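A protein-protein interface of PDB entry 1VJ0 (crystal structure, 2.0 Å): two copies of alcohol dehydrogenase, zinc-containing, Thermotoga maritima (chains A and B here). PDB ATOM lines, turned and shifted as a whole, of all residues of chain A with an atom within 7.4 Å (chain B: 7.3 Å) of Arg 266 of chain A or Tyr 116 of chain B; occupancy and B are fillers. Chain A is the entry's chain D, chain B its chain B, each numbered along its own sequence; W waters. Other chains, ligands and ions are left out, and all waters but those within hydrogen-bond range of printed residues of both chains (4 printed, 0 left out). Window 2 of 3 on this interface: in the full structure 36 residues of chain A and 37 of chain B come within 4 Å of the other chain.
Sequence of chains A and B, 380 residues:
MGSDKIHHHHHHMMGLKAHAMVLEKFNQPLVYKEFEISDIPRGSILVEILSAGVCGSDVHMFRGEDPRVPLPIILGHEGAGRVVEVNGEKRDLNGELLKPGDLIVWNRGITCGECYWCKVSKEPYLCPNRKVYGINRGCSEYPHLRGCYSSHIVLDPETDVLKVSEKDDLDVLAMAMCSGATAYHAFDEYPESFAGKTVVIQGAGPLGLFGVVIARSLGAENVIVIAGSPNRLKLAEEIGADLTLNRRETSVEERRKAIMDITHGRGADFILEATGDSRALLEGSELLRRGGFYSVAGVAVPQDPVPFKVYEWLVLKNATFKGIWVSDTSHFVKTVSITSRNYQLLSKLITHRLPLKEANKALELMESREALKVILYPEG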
ATOM      1  N   TYR A 190      24.792 -23.876  -4.048  1.00  0.00           N
ATOM      2  CA  TYR A 190      23.387 -24.042  -4.373  1.00  0.00           C
ATOM      3  C   TYR A 190      22.513 -23.322  -3.338  1.00  0.00           C
ATOM      4  O   TYR A 190      22.660 -23.585  -2.163  1.00  0.00           O
ATOM      5  CB  TYR A 190      23.035 -25.531  -4.404  1.00  0.00           C
ATOM      6  CG  TYR A 190      21.680 -25.845  -5.004  1.00  0.00           C
ATOM      7  CD1 TYR A 190      21.382 -25.508  -6.329  1.00  0.00           C
ATOM      8  CD2 TYR A 190      20.706 -26.497  -4.278  1.00  0.00           C
ATOM      9  CE1 TYR A 190      20.159 -25.789  -6.876  1.00  0.00           C
ATOM     10  CE2 TYR A 190      19.474 -26.815  -4.848  1.00  0.00           C
ATOM     11  CZ  TYR A 190      19.203 -26.449  -6.139  1.00  0.00           C
ATOM     12  OH  TYR A 190      17.974 -26.762  -6.717  1.00  0.00           O
ATOM     13  N   GLU A 192      19.370 -23.420  -2.353  1.00  0.00           N
ATOM     14  CA  GLU A 192      18.201 -24.066  -1.832  1.00  0.00           C
ATOM     15  C   GLU A 192      18.618 -25.369  -1.189  1.00  0.00           C
ATOM     16  O   GLU A 192      19.753 -25.830  -1.385  1.00  0.00           O
ATOM     17  CB  GLU A 192      17.299 -24.467  -2.997  1.00  0.00           C
ATOM     18  CG  GLU A 192      16.830 -23.347  -3.867  1.00  0.00           C
ATOM     19  CD  GLU A 192      15.501 -23.688  -4.504  1.00  0.00           C
ATOM     20  OE1 GLU A 192      14.985 -24.832  -4.301  1.00  0.00           O
ATOM     21  OE2 GLU A 192      14.952 -22.793  -5.191  1.00  0.00           O
ATOM     22  N   ALA A 195      16.451 -31.269  -0.931  1.00  0.00           N
ATOM     23  CA  ALA A 195      15.261 -32.115  -0.794  1.00  0.00           C
ATOM     24  C   ALA A 195      14.466 -32.084  -2.131  1.00  0.00           C
ATOM     25  O   ALA A 195      14.246 -31.027  -2.684  1.00  0.00           O
ATOM     26  CB  ALA A 195      14.387 -31.652   0.378  1.00  0.00           C
ATOM     27  N   GLY A 196      14.081 -33.244  -2.656  1.00  0.00           N
ATOM     28  CA  GLY A 196      13.264 -33.261  -3.839  1.00  0.00           C
ATOM     29  C   GLY A 196      13.993 -32.985  -5.140  1.00  0.00           C
ATOM     30  O   GLY A 196      13.354 -32.961  -6.195  1.00  0.00           O
ATOM     31  N   LYS A 197      15.310 -32.854  -5.086  1.00  0.00           N
ATOM     32  CA  LYS A 197      16.102 -32.429  -6.226  1.00  0.00           C
ATOM     33  C   LYS A 197      16.795 -33.589  -6.912  1.00  0.00           C
ATOM     34  O   LYS A 197      17.196 -34.578  -6.276  1.00  0.00           O
ATOM     35  CB  LYS A 197      17.142 -31.364  -5.831  1.00  0.00           C
ATOM     36  CG  LYS A 197      16.522 -30.061  -5.197  1.00  0.00           C
ATOM     37  CD  LYS A 197      15.607 -29.303  -6.143  1.00  0.00           C
ATOM     38  CE  LYS A 197      14.837 -28.129  -5.449  1.00  0.00           C
ATOM     39  NZ  LYS A 197      15.813 -27.190  -4.809  1.00  0.00           N
ATOM     40  N   THR A 198      16.915 -33.442  -8.225  1.00  0.00           N
ATOM     41  CA  THR A 198      17.699 -34.357  -9.072  1.00  0.00           C
ATOM     42  C   THR A 198      19.059 -33.745  -9.403  1.00  0.00           C
ATOM     43  O   THR A 198      19.146 -32.651  -9.992  1.00  0.00           O
ATOM     44  CB  THR A 198      16.971 -34.666 -10.365  1.00  0.00           C
ATOM     45  OG1 THR A 198      15.815 -35.429 -10.047  1.00  0.00           O
ATOM     46  CG2 THR A 198      17.812 -35.560 -11.273  1.00  0.00           C
ATOM     47  N   ARG A 256      19.801 -38.142 -22.317  1.00  0.00           N
ATOM     48  CA  ARG A 256      18.869 -37.062 -22.128  1.00  0.00           C
ATOM     49  C   ARG A 256      17.476 -37.627 -21.796  1.00  0.00           C
ATOM     50  O   ARG A 256      16.843 -37.179 -20.827  1.00  0.00           O
ATOM     51  CB  ARG A 256      18.845 -36.173 -23.371  1.00  0.00           C
ATOM     52  CG  ARG A 256      18.114 -34.884 -23.181  1.00  0.00           C
ATOM     53  CD  ARG A 256      18.158 -33.938 -24.388  1.00  0.00           C
ATOM     54  NE  ARG A 256      16.791 -33.454 -24.632  1.00  0.00           N
ATOM     55  CZ  ARG A 256      16.296 -32.311 -24.130  1.00  0.00           C
ATOM     56  NH1 ARG A 256      17.052 -31.495 -23.389  1.00  0.00           N
ATOM     57  NH2 ARG A 256      15.039 -31.972 -24.394  1.00  0.00           N
ATOM     58  N   ILE A 259      17.292 -38.832 -18.204  1.00  0.00           N
ATOM     59  CA  ILE A 259      17.194 -37.749 -17.229  1.00  0.00           C
ATOM     60  C   ILE A 259      15.814 -37.054 -17.261  1.00  0.00           C
ATOM     61  O   ILE A 259      15.244 -36.701 -16.198  1.00  0.00           O
ATOM     62  CB  ILE A 259      18.394 -36.808 -17.424  1.00  0.00           C
ATOM     63  CG1 ILE A 259      19.632 -37.555 -16.927  1.00  0.00           C
ATOM     64  CG2 ILE A 259      18.189 -35.511 -16.743  1.00  0.00           C
ATOM     65  CD1 ILE A 259      20.845 -36.989 -17.399  1.00  0.00           C
ATOM     66  N   MET A 260      15.280 -36.906 -18.477  1.00  0.00           N
ATOM     67  CA  MET A 260      13.985 -36.307 -18.706  1.00  0.00           C
ATOM     68  C   MET A 260      12.940 -37.225 -18.104  1.00  0.00           C
ATOM     69  O   MET A 260      12.039 -36.736 -17.484  1.00  0.00           O
ATOM     70  CB  MET A 260      13.709 -36.054 -20.199  1.00  0.00           C
ATOM     71  CG  MET A 260      14.476 -34.874 -20.862  1.00  0.00           C
ATOM     72  SD  MET A 260      14.637 -33.412 -19.823  1.00  0.00           S
ATOM     73  CE  MET A 260      16.308 -32.902 -20.188  1.00  0.00           C
ATOM     74  N   ASP A 261      13.085 -38.546 -18.222  1.00  0.00           N
ATOM     75  CA  ASP A 261      12.109 -39.459 -17.602  1.00  0.00           C
ATOM     76  C   ASP A 261      12.061 -39.333 -16.072  1.00  0.00           C
ATOM     77  O   ASP A 261      10.953 -39.306 -15.465  1.00  0.00           O
ATOM     78  CB  ASP A 261      12.433 -40.919 -17.892  1.00  0.00           C
ATOM     79  CG  ASP A 261      12.107 -41.341 -19.319  1.00  0.00           C
ATOM     80  OD1 ASP A 261      11.474 -40.566 -20.083  1.00  0.00           O
ATOM     81  OD2 ASP A 261      12.509 -42.458 -19.738  1.00  0.00           O
ATOM     82  N   ILE A 262      13.243 -39.286 -15.468  1.00  0.00           N
ATOM     83  CA  ILE A 262      13.406 -39.144 -14.029  1.00  0.00           C
ATOM     84  C   ILE A 262      12.863 -37.815 -13.473  1.00  0.00           C
ATOM     85  O   ILE A 262      12.442 -37.755 -12.301  1.00  0.00           O
ATOM     86  CB  ILE A 262      14.894 -39.293 -13.662  1.00  0.00           C
ATOM     87  CG1 ILE A 262      15.296 -40.750 -13.790  1.00  0.00           C
ATOM     88  CG2 ILE A 262      15.173 -38.772 -12.273  1.00  0.00           C
ATOM     89  CD1 ILE A 262      16.798 -41.005 -13.691  1.00  0.00           C
ATOM     90  N   THR A 263      12.901 -36.760 -14.301  1.00  0.00           N
ATOM     91  CA  THR A 263      12.582 -35.395 -13.869  1.00  0.00           C
ATOM     92  C   THR A 263      11.296 -34.866 -14.536  1.00  0.00           C
ATOM     93  O   THR A 263      11.127 -33.651 -14.658  1.00  0.00           O
ATOM     94  CB  THR A 263      13.718 -34.420 -14.208  1.00  0.00           C
ATOM     95  OG1 THR A 263      13.976 -34.463 -15.618  1.00  0.00           O
ATOM     96  CG2 THR A 263      15.026 -34.822 -13.540  1.00  0.00           C
ATOM     97  N   HIS A 264      10.452 -35.787 -15.011  1.00  0.00           N
ATOM     98  CA  HIS A 264       9.164 -35.472 -15.572  1.00  0.00           C
ATOM     99  C   HIS A 264       9.277 -34.450 -16.658  1.00  0.00           C
ATOM    100  O   HIS A 264       8.432 -33.578 -16.789  1.00  0.00           O
ATOM    101  CB  HIS A 264       8.214 -35.020 -14.471  1.00  0.00           C
ATOM    102  CG  HIS A 264       7.907 -36.104 -13.510  1.00  0.00           C
ATOM    103  ND1 HIS A 264       6.962 -37.063 -13.781  1.00  0.00           N
ATOM    104  CD2 HIS A 264       8.421 -36.400 -12.298  1.00  0.00           C
ATOM    105  CE1 HIS A 264       6.918 -37.915 -12.773  1.00  0.00           C
ATOM    106  NE2 HIS A 264       7.801 -37.538 -11.871  1.00  0.00           N
ATOM    107  N   GLY A 265      10.322 -34.586 -17.474  1.00  0.00           N
ATOM    108  CA  GLY A 265      10.508 -33.720 -18.623  1.00  0.00           C
ATOM    109  C   GLY A 265      11.164 -32.388 -18.364  1.00  0.00           C
ATOM    110  O   GLY A 265      11.265 -31.596 -19.253  1.00  0.00           O
ATOM    111  N   ARG A 266      11.605 -32.111 -17.147  1.00  0.00           N
ATOM    112  CA  ARG A 266      12.161 -30.792 -16.858  1.00  0.00           C
ATOM    113  C   ARG A 266      13.648 -30.711 -17.116  1.00  0.00           C
ATOM    114  O   ARG A 266      14.131 -29.682 -17.600  1.00  0.00           O
ATOM    115  CB  ARG A 266      11.929 -30.458 -15.382  1.00  0.00           C
ATOM    116  CG  ARG A 266      10.451 -30.379 -15.009  1.00  0.00           C
ATOM    117  CD  ARG A 266      10.230 -29.749 -13.705  1.00  0.00           C
ATOM    118  NE  ARG A 266      10.780 -30.560 -12.651  1.00  0.00           N
ATOM    119  CZ  ARG A 266      10.111 -31.494 -11.983  1.00  0.00           C
ATOM    120  NH1 ARG A 266       8.797 -31.745 -12.194  1.00  0.00           N
ATOM    121  NH2 ARG A 266      10.767 -32.140 -11.050  1.00  0.00           N
ATOM    122  N   GLY A 267      14.373 -31.772 -16.757  1.00  0.00           N
ATOM    123  CA  GLY A 267      15.789 -31.739 -16.630  1.00  0.00           C
ATOM    124  C   GLY A 267      16.260 -31.713 -15.182  1.00  0.00           C
ATOM    125  O   GLY A 267      15.468 -31.566 -14.223  1.00  0.00           O
ATOM    126  N   ALA A 268      17.569 -31.826 -15.033  1.00  0.00           N
ATOM    127  CA  ALA A 268      18.210 -31.832 -13.721  1.00  0.00           C
ATOM    128  C   ALA A 268      18.175 -30.487 -13.034  1.00  0.00           C
ATOM    129  O   ALA A 268      18.252 -29.398 -13.688  1.00  0.00           O
ATOM    130  CB  ALA A 268      19.639 -32.303 -13.853  1.00  0.00           C
ATOM    131  N   ASP A 269      18.084 -30.554 -11.702  1.00  0.00           N
ATOM    132  CA  ASP A 269      18.042 -29.336 -10.895  1.00  0.00           C
ATOM    133  C   ASP A 269      19.433 -28.723 -10.672  1.00  0.00           C
ATOM    134  O   ASP A 269      19.587 -27.497 -10.643  1.00  0.00           O
ATOM    135  CB  ASP A 269      17.394 -29.656  -9.555  1.00  0.00           C
ATOM    136  CG  ASP A 269      15.969 -30.150  -9.742  1.00  0.00           C
ATOM    137  OD1 ASP A 269      15.180 -29.449 -10.425  1.00  0.00           O
ATOM    138  OD2 ASP A 269      15.571 -31.238  -9.316  1.00  0.00           O
ATOM    139  N   GLU A 286      22.353 -29.192 -21.996  1.00  0.00           N
ATOM    140  CA  GLU A 286      21.113 -29.711 -22.542  1.00  0.00           C
ATOM    141  C   GLU A 286      20.351 -30.577 -21.534  1.00  0.00           C
ATOM    142  O   GLU A 286      19.185 -30.840 -21.732  1.00  0.00           O
ATOM    143  CB  GLU A 286      21.372 -30.471 -23.860  1.00  0.00           C
ATOM    144  CG  GLU A 286      22.120 -29.633 -24.931  1.00  0.00           C
ATOM    145  CD  GLU A 286      21.310 -28.464 -25.537  1.00  0.00           C
ATOM    146  OE1 GLU A 286      20.123 -28.252 -25.197  1.00  0.00           O
ATOM    147  OE2 GLU A 286      21.875 -27.719 -26.399  1.00  0.00           O
ATOM    148  N   LEU A 287      20.996 -30.960 -20.433  1.00  0.00           N
ATOM    149  CA  LEU A 287      20.357 -31.746 -19.372  1.00  0.00           C
ATOM    150  C   LEU A 287      19.765 -30.886 -18.218  1.00  0.00           C
ATOM    151  O   LEU A 287      19.106 -31.416 -17.333  1.00  0.00           O
ATOM    152  CB  LEU A 287      21.395 -32.709 -18.754  1.00  0.00           C
ATOM    153  CG  LEU A 287      21.961 -33.786 -19.659  1.00  0.00           C
ATOM    154  CD1 LEU A 287      22.973 -34.625 -18.856  1.00  0.00           C
ATOM    155  CD2 LEU A 287      20.880 -34.686 -20.304  1.00  0.00           C
ATOM    156  N   LEU A 288      20.076 -29.591 -18.222  1.00  0.00           N
ATOM    157  CA  LEU A 288      19.777 -28.716 -17.125  1.00  0.00           C
ATOM    158  C   LEU A 288      18.365 -28.179 -17.319  1.00  0.00           C
ATOM    159  O   LEU A 288      18.014 -27.756 -18.413  1.00  0.00           O
ATOM    160  CB  LEU A 288      20.833 -27.609 -17.140  1.00  0.00           C
ATOM    161  CG  LEU A 288      20.837 -26.684 -15.916  1.00  0.00           C
ATOM    162  CD1 LEU A 288      21.291 -27.488 -14.714  1.00  0.00           C
ATOM    163  CD2 LEU A 288      21.726 -25.462 -16.203  1.00  0.00           C
ATOM    164  N   ARG A 289      17.529 -28.251 -16.283  1.00  0.00           N
ATOM    165  CA  ARG A 289      16.203 -27.621 -16.345  1.00  0.00           C
ATOM    166  C   ARG A 289      16.264 -26.122 -16.454  1.00  0.00           C
ATOM    167  O   ARG A 289      17.266 -25.497 -16.053  1.00  0.00           O
ATOM    168  CB  ARG A 289      15.334 -27.981 -15.151  1.00  0.00           C
ATOM    169  CG  ARG A 289      15.650 -27.318 -13.827  1.00  0.00           C
ATOM    170  CD  ARG A 289      14.383 -27.350 -12.960  1.00  0.00           C
ATOM    171  NE  ARG A 289      14.616 -26.957 -11.584  1.00  0.00           N
ATOM    172  CZ  ARG A 289      14.443 -25.748 -11.070  1.00  0.00           C
ATOM    173  NH1 ARG A 289      14.094 -24.677 -11.802  1.00  0.00           N
ATOM    174  NH2 ARG A 289      14.572 -25.625  -9.770  1.00  0.00           N
ATOM    175  N   ARG A 290      15.169 -25.540 -16.943  1.00  0.00           N
ATOM    176  CA  ARG A 290      15.025 -24.089 -16.864  1.00  0.00           C
ATOM    177  C   ARG A 290      15.064 -23.707 -15.419  1.00  0.00           C
ATOM    178  O   ARG A 290      14.366 -24.330 -14.590  1.00  0.00           O
ATOM    179  CB  ARG A 290      13.735 -23.596 -17.498  1.00  0.00           C
ATOM    180  CG  ARG A 290      13.644 -23.864 -19.008  1.00  0.00           C
ATOM    181  CD  ARG A 290      12.385 -23.328 -19.590  1.00  0.00           C
ATOM    182  NE  ARG A 290      12.579 -21.904 -19.913  1.00  0.00           N
ATOM    183  CZ  ARG A 290      11.625 -20.999 -20.035  1.00  0.00           C
ATOM    184  NH1 ARG A 290      10.341 -21.281 -19.844  1.00  0.00           N
ATOM    185  NH2 ARG A 290      11.961 -19.764 -20.360  1.00  0.00           N
ATOM    186  N   LYS A 317      16.991 -20.366 -20.584  1.00  0.00           N
ATOM    187  CA  LYS A 317      16.940 -21.318 -19.525  1.00  0.00           C
ATOM    188  C   LYS A 317      16.918 -20.644 -18.152  1.00  0.00           C
ATOM    189  O   LYS A 317      16.639 -21.300 -17.156  1.00  0.00           O
ATOM    190  CB  LYS A 317      18.182 -22.235 -19.643  1.00  0.00           C
ATOM    191  CG  LYS A 317      18.083 -23.568 -19.002  1.00  0.00           C
ATOM    192  CD  LYS A 317      19.270 -24.503 -19.274  1.00  0.00           C
ATOM    193  CE  LYS A 317      19.151 -25.155 -20.653  1.00  0.00           C
ATOM    194  NZ  LYS A 317      18.500 -26.442 -20.630  1.00  0.00           N
ATOM    195  N   CYS B 112       0.180 -20.198 -15.243  1.00  0.00           N
ATOM    196  CA  CYS B 112      -0.855 -21.186 -14.987  1.00  0.00           C
ATOM    197  C   CYS B 112      -1.131 -21.338 -13.500  1.00  0.00           C
ATOM    198  O   CYS B 112      -2.220 -21.787 -13.131  1.00  0.00           O
ATOM    199  CB  CYS B 112      -0.472 -22.547 -15.624  1.00  0.00           C
ATOM    200  SG  CYS B 112       0.811 -23.556 -14.781  1.00  0.00           S
ATOM    201  N   GLU B 114      -0.177 -23.630 -11.553  1.00  0.00           N
ATOM    202  CA  GLU B 114      -0.270 -25.041 -11.167  1.00  0.00           C
ATOM    203  C   GLU B 114       0.951 -25.904 -11.442  1.00  0.00           C
ATOM    204  O   GLU B 114       1.032 -27.001 -10.925  1.00  0.00           O
ATOM    205  CB  GLU B 114      -1.540 -25.684 -11.750  1.00  0.00           C
ATOM    206  CG  GLU B 114      -1.706 -25.540 -13.244  1.00  0.00           C
ATOM    207  CD  GLU B 114      -3.043 -26.118 -13.766  1.00  0.00           C
ATOM    208  OE1 GLU B 114      -4.117 -25.467 -13.617  1.00  0.00           O
ATOM    209  OE2 GLU B 114      -2.996 -27.221 -14.350  1.00  0.00           O
ATOM    210  N   CYS B 115       1.917 -25.403 -12.207  1.00  0.00           N
ATOM    211  CA  CYS B 115       3.049 -26.255 -12.636  1.00  0.00           C
ATOM    212  C   CYS B 115       4.215 -26.196 -11.648  1.00  0.00           C
ATOM    213  O   CYS B 115       4.155 -25.485 -10.637  1.00  0.00           O
ATOM    214  CB  CYS B 115       3.538 -25.787 -14.006  1.00  0.00           C
ATOM    215  SG  CYS B 115       4.373 -24.185 -13.943  1.00  0.00           S
ATOM    216  N   TYR B 116       5.275 -26.957 -11.944  1.00  0.00           N
ATOM    217  CA  TYR B 116       6.450 -27.009 -11.077  1.00  0.00           C
ATOM    218  C   TYR B 116       7.047 -25.644 -10.796  1.00  0.00           C
ATOM    219  O   TYR B 116       7.350 -25.290  -9.649  1.00  0.00           O
ATOM    220  CB  TYR B 116       7.507 -27.933 -11.666  1.00  0.00           C
ATOM    221  CG  TYR B 116       8.787 -28.001 -10.864  1.00  0.00           C
ATOM    222  CD1 TYR B 116       9.826 -27.133 -11.128  1.00  0.00           C
ATOM    223  CD2 TYR B 116       8.976 -28.969  -9.874  1.00  0.00           C
ATOM    224  CE1 TYR B 116      11.057 -27.212 -10.434  1.00  0.00           C
ATOM    225  CE2 TYR B 116      10.201 -29.048  -9.173  1.00  0.00           C
ATOM    226  CZ  TYR B 116      11.222 -28.135  -9.455  1.00  0.00           C
ATOM    227  OH  TYR B 116      12.423 -28.167  -8.773  1.00  0.00           O
ATOM    228  N   TRP B 117       7.153 -24.825 -11.834  1.00  0.00           N
ATOM    229  CA  TRP B 117       7.753 -23.519 -11.666  1.00  0.00           C
ATOM    230  C   TRP B 117       6.856 -22.500 -10.934  1.00  0.00           C
ATOM    231  O   TRP B 117       7.350 -21.721 -10.143  1.00  0.00           O
ATOM    232  CB  TRP B 117       8.237 -22.982 -13.003  1.00  0.00           C
ATOM    233  CG  TRP B 117       9.324 -23.783 -13.641  1.00  0.00           C
ATOM    234  CD1 TRP B 117      10.653 -23.605 -13.478  1.00  0.00           C
ATOM    235  CD2 TRP B 117       9.179 -24.842 -14.582  1.00  0.00           C
ATOM    236  NE1 TRP B 117      11.355 -24.525 -14.209  1.00  0.00           N
ATOM    237  CE2 TRP B 117      10.469 -25.278 -14.930  1.00  0.00           C
ATOM    238  CE3 TRP B 117       8.084 -25.492 -15.153  1.00  0.00           C
ATOM    239  CZ2 TRP B 117      10.690 -26.326 -15.803  1.00  0.00           C
ATOM    240  CZ3 TRP B 117       8.309 -26.530 -16.017  1.00  0.00           C
ATOM    241  CH2 TRP B 117       9.587 -26.921 -16.359  1.00  0.00           C
ATOM    242  N   CYS B 118       5.549 -22.522 -11.169  1.00  0.00           N
ATOM    243  CA  CYS B 118       4.651 -21.616 -10.476  1.00  0.00           C
ATOM    244  C   CYS B 118       4.498 -21.964  -8.991  1.00  0.00           C
ATOM    245  O   CYS B 118       4.372 -21.074  -8.137  1.00  0.00           O
ATOM    246  CB  CYS B 118       3.261 -21.612 -11.138  1.00  0.00           C
ATOM    247  SG  CYS B 118       3.193 -20.873 -12.827  1.00  0.00           S
ATOM    248  N   LYS B 119       4.468 -23.241  -8.665  1.00  0.00           N
ATOM    249  CA  LYS B 119       4.105 -23.691  -7.319  1.00  0.00           C
ATOM    250  C   LYS B 119       5.216 -24.344  -6.504  1.00  0.00           C
ATOM    251  O   LYS B 119       5.105 -24.427  -5.285  1.00  0.00           O
ATOM    252  CB  LYS B 119       2.951 -24.702  -7.414  1.00  0.00           C
ATOM    253  CG  LYS B 119       1.551 -24.071  -7.579  1.00  0.00           C
ATOM    254  CD  LYS B 119       1.081 -23.448  -6.277  1.00  0.00           C
ATOM    255  CE  LYS B 119      -0.373 -22.896  -6.301  1.00  0.00           C
ATOM    256  NZ  LYS B 119      -1.301 -23.888  -6.844  1.00  0.00           N
ATOM    257  N   VAL B 120       6.217 -24.929  -7.155  1.00  0.00           N
ATOM    258  CA  VAL B 120       7.251 -25.661  -6.437  1.00  0.00           C
ATOM    259  C   VAL B 120       8.527 -24.797  -6.356  1.00  0.00           C
ATOM    260  O   VAL B 120       8.976 -24.468  -5.245  1.00  0.00           O
ATOM    261  CB  VAL B 120       7.491 -27.055  -7.007  1.00  0.00           C
ATOM    262  CG1 VAL B 120       8.564 -27.824  -6.179  1.00  0.00           C
ATOM    263  CG2 VAL B 120       6.175 -27.871  -6.988  1.00  0.00           C
ATOM    264  N   SER B 121       9.100 -24.419  -7.502  1.00  0.00           N
ATOM    265  CA  SER B 121      10.336 -23.636  -7.470  1.00  0.00           C
ATOM    266  C   SER B 121      10.090 -22.103  -7.319  1.00  0.00           C
ATOM    267  O   SER B 121      11.020 -21.332  -7.060  1.00  0.00           O
ATOM    268  CB  SER B 121      11.191 -23.973  -8.691  1.00  0.00           C
ATOM    269  OG  SER B 121      10.613 -23.395  -9.842  1.00  0.00           O
ATOM    270  N   LYS B 122       8.844 -21.676  -7.426  1.00  0.00           N
ATOM    271  CA  LYS B 122       8.467 -20.289  -7.285  1.00  0.00           C
ATOM    272  C   LYS B 122       9.219 -19.386  -8.276  1.00  0.00           C
ATOM    273  O   LYS B 122       9.669 -18.305  -7.915  1.00  0.00           O
ATOM    274  CB  LYS B 122       8.633 -19.804  -5.821  1.00  0.00           C
ATOM    275  CG  LYS B 122       7.794 -20.588  -4.822  1.00  0.00           C
ATOM    276  CD  LYS B 122       7.973 -20.070  -3.368  1.00  0.00           C
ATOM    277  CE  LYS B 122       7.152 -20.896  -2.427  1.00  0.00           C
ATOM    278  NZ  LYS B 122       7.392 -20.496  -0.993  1.00  0.00           N
ATOM    279  N   GLU B 123       9.288 -19.839  -9.529  1.00  0.00           N
ATOM    280  CA  GLU B 123       9.901 -19.112 -10.642  1.00  0.00           C
ATOM    281  C   GLU B 123       8.828 -18.955 -11.757  1.00  0.00           C
ATOM    282  O   GLU B 123       8.912 -19.538 -12.796  1.00  0.00           O
ATOM    283  CB  GLU B 123      11.115 -19.868 -11.137  1.00  0.00           C
ATOM    284  CG  GLU B 123      12.235 -20.102 -10.106  1.00  0.00           C
ATOM    285  CD  GLU B 123      13.241 -21.227 -10.462  1.00  0.00           C
ATOM    286  OE1 GLU B 123      12.888 -22.338 -10.971  1.00  0.00           O
ATOM    287  OE2 GLU B 123      14.426 -21.033 -10.168  1.00  0.00           O
ATOM    288  N   PRO B 128       5.888 -22.754 -18.454  1.00  0.00           N
ATOM    289  CA  PRO B 128       5.786 -23.099 -19.855  1.00  0.00           C
ATOM    290  C   PRO B 128       4.429 -22.728 -20.466  1.00  0.00           C
ATOM    291  O   PRO B 128       4.252 -22.865 -21.665  1.00  0.00           O
ATOM    292  CB  PRO B 128       5.974 -24.626 -19.837  1.00  0.00           C
ATOM    293  CG  PRO B 128       5.497 -25.032 -18.592  1.00  0.00           C
ATOM    294  CD  PRO B 128       5.844 -23.954 -17.610  1.00  0.00           C
HETATM  295  O   HOH W   1      12.971 -31.090  -8.880  1.00  0.00           O
HETATM  296  O   HOH W   2      12.635 -21.938  -5.181  1.00  0.00           O
HETATM  297  O   HOH W   3      15.068 -22.975  -8.627  1.00  0.00           O
HETATM  298  O   HOH W   4      12.121 -24.929  -4.355  1.00  0.00           O
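Arg 266 of chain A touches two residues of chain B. Tyr 116 of chain B touches just these residues of chain A: Arg 266 (3.5 Å), Asp 269 (3.5 Å) and Arg 289 (3.5 Å). No residue of chain B comes within 4 Å of Gly 265 of chain A. Of the printed residues of chain A, Ser 121 of chain B touches Arg 289. Printed residues of chain B within 4 Å of Arg 290 of chain A: Trp 117 (3.0 Å). Glu 286 of chain A touches none of the printed residues of chain B.
CZ of Arg 266 of chain A touches CD2 of Tyr 116 of chain B, 3.5 Å away. CG of Arg 266 of chain A touches CH2 of Trp 117 of chain B, at 3.8 Å. NH1 of Arg 289 of chain A touches NE1 of Trp 117 of chain B, at 3.6 Å. Arg 289 of chain A touches Ser 121 of chain B.
Printed residues of chain B that touch a printed residue of chain A: Tyr 116, Trp 117, Ser 121 and Glu 123. Hydrophobic or aromatic side chains of chain B within 4 Å of the printed part of chain A: Tyr 116 and Trp 117. Among the printed residues, 8 pairs touch across the chains. Among the printed residues, Asp or Glu carboxylates within 4 Å of a Lys or Arg side-chain nitrogen of the other chain: Arg 289 of chain A with Glu 123 of chain B (2.8 Å).
No position is printed for both chains. Of the 8 pairs that touch across the chains among the printed residues, none has its exchanged pair printed and touching as well.
The backbone NH (N) of Thr 198 of chain A lies within hydrogen-bond range of the side-chain carboxylate (OD2) of Asp 269 of chain A. The side-chain sulfur (SG) of Cys 115 of chain B lies close to the backbone NH (N) of Trp 117 of chain B, at 3.5 Å. OG of Ser 121 of chain B sits at hydrogen-bond distance from OE1 of Glu 123 of chain B, 2.8 Å away. O of Tyr 116 of chain B sits at hydrogen-bond distance from N of Ser 121 of chain B (2.9 Å). N of Arg 289 of chain A lies within hydrogen-bond range of O of Ala 268 of chain A (2.9 Å). The backbone carbonyl oxygen (O) of Trp 117 of chain B sits at hydrogen-bond distance from the backbone NH (N) of Lys 122 of chain B.
The side-chain carboxylate (OE1) of Glu 123 of chain B is in salt-bridge range of the guanidinium group (NH1) of Arg 289 of chain A, at 2.8 Å. OH of Tyr 116 of chain B is in hydrogen-bond range of NH2 of Arg 289 of chain A, 3.5 Å away. The indole nitrogen of Trp 117 of chain B lies within hydrogen-bond range of the backbone carbonyl oxygen of Arg 290 of chain A (3.0 Å). The side-chain hydroxyl (OH) of Tyr 116 of chain B sits at hydrogen-bond distance from the side-chain carboxylate (OD1) of Asp 269 of chain A, 3.5 Å away.
Water W2 lies within hydrogen-bond range of the side-chain carboxylate (OE2) of Glu 192 of chain A (2.5 Å) and the backbone carbonyl oxygen (O) of Ser 121 of chain B (2.6 Å). Water W1 lies within hydrogen-bond range of OD2 of Asp 269 of chain A (2.6 Å), OH of Tyr 116 of chain B (3.0 Å), NH2 of Arg 266 of chain A (3.3 Å) and O of Gly 196 of chain A (3.3 Å). Water W4 lies within hydrogen-bond range of the side-chain carboxylate of Glu 192 of chain A (2.9 Å) and the backbone carbonyl oxygen of Val 120 of chain B (3.3 Å).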
